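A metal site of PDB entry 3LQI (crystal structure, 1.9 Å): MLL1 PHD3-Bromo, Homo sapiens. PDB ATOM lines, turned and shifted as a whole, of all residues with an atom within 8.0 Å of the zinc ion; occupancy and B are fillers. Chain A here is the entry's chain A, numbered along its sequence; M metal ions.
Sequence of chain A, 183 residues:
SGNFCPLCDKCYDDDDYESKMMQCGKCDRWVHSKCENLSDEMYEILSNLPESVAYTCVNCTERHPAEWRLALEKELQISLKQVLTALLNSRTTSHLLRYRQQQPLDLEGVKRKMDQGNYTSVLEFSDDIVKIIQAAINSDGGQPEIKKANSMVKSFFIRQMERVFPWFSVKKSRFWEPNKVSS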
ATOM      1  N   PRO A   6       6.927 -30.761  21.046  1.00  0.00           N
ATOM      2  CA  PRO A   6       6.811 -31.800  22.068  1.00  0.00           C
ATOM      3  C   PRO A   6       6.420 -33.199  21.586  1.00  0.00           C
ATOM      4  O   PRO A   6       6.596 -34.170  22.320  1.00  0.00           O
ATOM      5  CB  PRO A   6       5.802 -31.225  23.057  1.00  0.00           C
ATOM      6  CG  PRO A   6       4.956 -30.300  22.202  1.00  0.00           C
ATOM      7  CD  PRO A   6       6.003 -29.635  21.323  1.00  0.00           C
ATOM      8  N   GLN A  23       0.603 -22.740  18.736  1.00  0.00           N
ATOM      9  CA  GLN A  23       1.330 -22.539  19.984  1.00  0.00           C
ATOM     10  C   GLN A  23       0.428 -22.776  21.181  1.00  0.00           C
ATOM     11  O   GLN A  23      -0.625 -22.148  21.312  1.00  0.00           O
ATOM     12  CB  GLN A  23       1.935 -21.131  20.044  1.00  0.00           C
ATOM     13  CG  GLN A  23       2.771 -20.904  21.297  1.00  0.00           C
ATOM     14  CD  GLN A  23       3.398 -19.526  21.356  1.00  0.00           C
ATOM     15  OE1 GLN A  23       2.775 -18.528  21.003  1.00  0.00           O
ATOM     16  NE2 GLN A  23       4.640 -19.460  21.841  1.00  0.00           N
ATOM     17  N   CYS A  24       0.847 -23.688  22.054  1.00  0.00           N
ATOM     18  CA  CYS A  24       0.072 -23.999  23.247  1.00  0.00           C
ATOM     19  C   CYS A  24       0.013 -22.793  24.165  1.00  0.00           C
ATOM     20  O   CYS A  24       1.045 -22.208  24.511  1.00  0.00           O
ATOM     21  CB  CYS A  24       0.683 -25.181  24.007  1.00  0.00           C
ATOM     22  SG  CYS A  24      -0.199 -25.585  25.538  1.00  0.00           S
ATOM     23  N   GLY A  25      -1.200 -22.427  24.570  1.00  0.00           N
ATOM     24  CA  GLY A  25      -1.377 -21.284  25.433  1.00  0.00           C
ATOM     25  C   GLY A  25      -0.878 -21.479  26.854  1.00  0.00           C
ATOM     26  O   GLY A  25      -0.740 -20.513  27.586  1.00  0.00           O
ATOM     27  N   LYS A  26      -0.596 -22.723  27.239  1.00  0.00           N
ATOM     28  CA  LYS A  26      -0.130 -22.981  28.586  1.00  0.00           C
ATOM     29  C   LYS A  26       1.379 -23.127  28.764  1.00  0.00           C
ATOM     30  O   LYS A  26       1.949 -22.557  29.687  1.00  0.00           O
ATOM     31  CB  LYS A  26      -0.852 -24.209  29.148  1.00  0.00           C
ATOM     32  CG  LYS A  26      -2.357 -24.055  29.118  1.00  0.00           C
ATOM     33  CD  LYS A  26      -3.061 -24.957  30.103  1.00  0.00           C
ATOM     34  CE  LYS A  26      -4.562 -24.678  30.084  1.00  0.00           C
ATOM     35  NZ  LYS A  26      -4.868 -23.224  30.287  1.00  0.00           N
ATOM     36  N   CYS A  27       2.032 -23.878  27.881  1.00  0.00           N
ATOM     37  CA  CYS A  27       3.471 -24.073  27.992  1.00  0.00           C
ATOM     38  C   CYS A  27       4.263 -23.285  26.948  1.00  0.00           C
ATOM     39  O   CYS A  27       5.494 -23.302  26.965  1.00  0.00           O
ATOM     40  CB  CYS A  27       3.812 -25.552  27.845  1.00  0.00           C
ATOM     41  SG  CYS A  27       3.564 -26.160  26.161  1.00  0.00           S
ATOM     42  N   ASP A  28       3.555 -22.622  26.048  1.00  0.00           N
ATOM     43  CA  ASP A  28       4.164 -21.810  24.991  1.00  0.00           C
ATOM     44  C   ASP A  28       4.921 -22.575  23.901  1.00  0.00           C
ATOM     45  O   ASP A  28       5.542 -21.956  23.028  1.00  0.00           O
ATOM     46  CB  ASP A  28       5.119 -20.768  25.597  1.00  0.00           C
ATOM     47  CG  ASP A  28       4.391 -19.735  26.433  1.00  0.00           C
ATOM     48  OD1 ASP A  28       3.366 -19.196  25.965  1.00  0.00           O
ATOM     49  OD2 ASP A  28       4.848 -19.444  27.554  1.00  0.00           O
ATOM     50  N   ARG A  29       4.873 -23.904  23.934  1.00  0.00           N
ATOM     51  CA  ARG A  29       5.561 -24.702  22.920  1.00  0.00           C
ATOM     52  C   ARG A  29       4.754 -24.716  21.621  1.00  0.00           C
ATOM     53  O   ARG A  29       3.521 -24.609  21.645  1.00  0.00           O
ATOM     54  CB  ARG A  29       5.767 -26.143  23.405  1.00  0.00           C
ATOM     55  CG  ARG A  29       6.707 -26.280  24.617  1.00  0.00           C
ATOM     56  CD  ARG A  29       8.175 -26.137  24.212  1.00  0.00           C
ATOM     57  NE  ARG A  29       8.709 -27.353  23.598  1.00  0.00           N
ATOM     58  CZ  ARG A  29       9.082 -28.442  24.273  1.00  0.00           C
ATOM     59  NH1 ARG A  29       8.976 -28.468  25.601  1.00  0.00           N
ATOM     60  NH2 ARG A  29       9.541 -29.507  23.628  1.00  0.00           N
ATOM     61  N   TRP A  30       5.436 -24.857  20.484  1.00  0.00           N
ATOM     62  CA  TRP A  30       4.772 -24.928  19.197  1.00  0.00           C
ATOM     63  C   TRP A  30       4.679 -26.385  18.793  1.00  0.00           C
ATOM     64  O   TRP A  30       5.623 -27.158  18.981  1.00  0.00           O
ATOM     65  CB  TRP A  30       5.544 -24.147  18.118  1.00  0.00           C
ATOM     66  CG  TRP A  30       5.448 -22.657  18.270  1.00  0.00           C
ATOM     67  CD1 TRP A  30       6.259 -21.853  19.021  1.00  0.00           C
ATOM     68  CD2 TRP A  30       4.486 -21.788  17.659  1.00  0.00           C
ATOM     69  NE1 TRP A  30       5.871 -20.552  18.911  1.00  0.00           N
ATOM     70  CE2 TRP A  30       4.789 -20.470  18.078  1.00  0.00           C
ATOM     71  CE3 TRP A  30       3.413 -21.998  16.786  1.00  0.00           C
ATOM     72  CZ2 TRP A  30       4.033 -19.368  17.664  1.00  0.00           C
ATOM     73  CZ3 TRP A  30       2.671 -20.899  16.376  1.00  0.00           C
ATOM     74  CH2 TRP A  30       2.982 -19.600  16.818  1.00  0.00           C
ATOM     75  N   VAL A  31       3.547 -26.755  18.221  1.00  0.00           N
ATOM     76  CA  VAL A  31       3.310 -28.129  17.789  1.00  0.00           C
ATOM     77  C   VAL A  31       2.882 -28.137  16.322  1.00  0.00           C
ATOM     78  O   VAL A  31       2.024 -27.362  15.926  1.00  0.00           O
ATOM     79  CB  VAL A  31       2.183 -28.757  18.643  1.00  0.00           C
ATOM     80  CG1 VAL A  31       1.857 -30.158  18.151  1.00  0.00           C
ATOM     81  CG2 VAL A  31       2.608 -28.770  20.098  1.00  0.00           C
ATOM     82  N   TYR A  55      -5.342 -23.116  21.822  1.00  0.00           N
ATOM     83  CA  TYR A  55      -4.860 -24.417  21.423  1.00  0.00           C
ATOM     84  C   TYR A  55      -4.112 -24.898  22.669  1.00  0.00           C
ATOM     85  O   TYR A  55      -3.484 -24.102  23.356  1.00  0.00           O
ATOM     86  CB  TYR A  55      -3.866 -24.318  20.264  1.00  0.00           C
ATOM     87  CG  TYR A  55      -3.032 -25.580  20.095  1.00  0.00           C
ATOM     88  CD1 TYR A  55      -3.616 -26.768  19.655  1.00  0.00           C
ATOM     89  CD2 TYR A  55      -1.680 -25.585  20.455  1.00  0.00           C
ATOM     90  CE1 TYR A  55      -2.873 -27.952  19.587  1.00  0.00           C
ATOM     91  CE2 TYR A  55      -0.934 -26.776  20.393  1.00  0.00           C
ATOM     92  CZ  TYR A  55      -1.537 -27.943  19.960  1.00  0.00           C
ATOM     93  OH  TYR A  55      -0.808 -29.116  19.919  1.00  0.00           O
ATOM     94  N   THR A  56      -4.196 -26.185  22.964  1.00  0.00           N
ATOM     95  CA  THR A  56      -3.485 -26.747  24.111  1.00  0.00           C
ATOM     96  C   THR A  56      -2.863 -28.034  23.601  1.00  0.00           C
ATOM     97  O   THR A  56      -3.540 -28.837  22.956  1.00  0.00           O
ATOM     98  CB  THR A  56      -4.427 -27.046  25.300  1.00  0.00           C
ATOM     99  OG1 THR A  56      -5.458 -27.962  24.877  1.00  0.00           O
ATOM    100  CG2 THR A  56      -5.068 -25.767  25.811  1.00  0.00           C
ATOM    101  N   CYS A  57      -1.580 -28.227  23.858  1.00  0.00           N
ATOM    102  CA  CYS A  57      -0.885 -29.421  23.401  1.00  0.00           C
ATOM    103  C   CYS A  57      -1.328 -30.644  24.188  1.00  0.00           C
ATOM    104  O   CYS A  57      -2.050 -30.529  25.180  1.00  0.00           O
ATOM    105  CB  CYS A  57       0.627 -29.239  23.531  1.00  0.00           C
ATOM    106  SG  CYS A  57       1.237 -29.276  25.233  1.00  0.00           S
ATOM    107  N   VAL A  58      -0.897 -31.824  23.757  1.00  0.00           N
ATOM    108  CA  VAL A  58      -1.250 -33.069  24.432  1.00  0.00           C
ATOM    109  C   VAL A  58      -0.835 -33.081  25.896  1.00  0.00           C
ATOM    110  O   VAL A  58      -1.527 -33.665  26.736  1.00  0.00           O
ATOM    111  CB  VAL A  58      -0.610 -34.291  23.736  1.00  0.00           C
ATOM    112  CG1 VAL A  58      -1.212 -34.470  22.359  1.00  0.00           C
ATOM    113  CG2 VAL A  58       0.895 -34.094  23.622  1.00  0.00           C
ATOM    114  N   ASN A  59       0.283 -32.444  26.205  1.00  0.00           N
ATOM    115  CA  ASN A  59       0.799 -32.399  27.573  1.00  0.00           C
ATOM    116  C   ASN A  59       0.012 -31.475  28.496  1.00  0.00           C
ATOM    117  O   ASN A  59      -0.117 -31.751  29.695  1.00  0.00           O
ATOM    118  CB  ASN A  59       2.254 -31.965  27.559  1.00  0.00           C
ATOM    119  CG  ASN A  59       3.150 -32.944  26.829  1.00  0.00           C
ATOM    120  OD1 ASN A  59       4.069 -32.555  26.121  1.00  0.00           O
ATOM    121  ND2 ASN A  59       2.887 -34.232  27.009  1.00  0.00           N
ATOM    122  N   CYS A  60      -0.514 -30.395  27.950  1.00  0.00           N
ATOM    123  CA  CYS A  60      -1.250 -29.425  28.773  1.00  0.00           C
ATOM    124  C   CYS A  60      -2.755 -29.556  28.756  1.00  0.00           C
ATOM    125  O   CYS A  60      -3.463 -28.829  29.444  1.00  0.00           O
ATOM    126  CB  CYS A  60      -0.823 -28.010  28.364  1.00  0.00           C
ATOM    127  SG  CYS A  60       0.957 -27.732  28.594  1.00  0.00           S
ATOM    128  N   THR A  61      -3.268 -30.488  27.959  1.00  0.00           N
ATOM    129  CA  THR A  61      -4.710 -30.702  27.871  1.00  0.00           C
ATOM    130  C   THR A  61      -5.114 -31.604  29.042  1.00  0.00           C
ATOM    131  O   THR A  61      -4.662 -32.746  29.118  1.00  0.00           O
ATOM    132  CB  THR A  61      -5.079 -31.393  26.529  1.00  0.00           C
ATOM    133  OG1 THR A  61      -4.651 -30.566  25.442  1.00  0.00           O
ATOM    134  CG2 THR A  61      -6.581 -31.621  26.440  1.00  0.00           C
HETATM  135 ZN    ZN M   1       1.442 -27.161  26.344  1.00  0.00          ZN
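O of Arg 29 lies within hydrogen-bond range of N of Cys 24 (2.9 Å).
SG of Cys 57 sits close to N of Asn 59, 3.4 Å away.
The side-chain sulfur (SG) of Cys 27 lies close to the backbone NH (N) of Arg 29 (3.4 Å).
The side-chain hydroxyl of Thr 61 lies within hydrogen-bond range of the backbone carbonyl oxygen of Cys 57, at 2.6 Å.
N of Lys 26 sits close to SG of Cys 24 (3.4 Å).
The nearest printed residue that does not touch the zinc ion is Lys 26 (4.7 Å).
The zinc ion is bound by the side-chain sulfur of Cys 27 (2.4 Å), the side-chain sulfur of Cys 60 (2.4 Å), the side-chain sulfur of Cys 57 (2.4 Å) and the side-chain sulfur of Cys 24 (2.4 Å).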
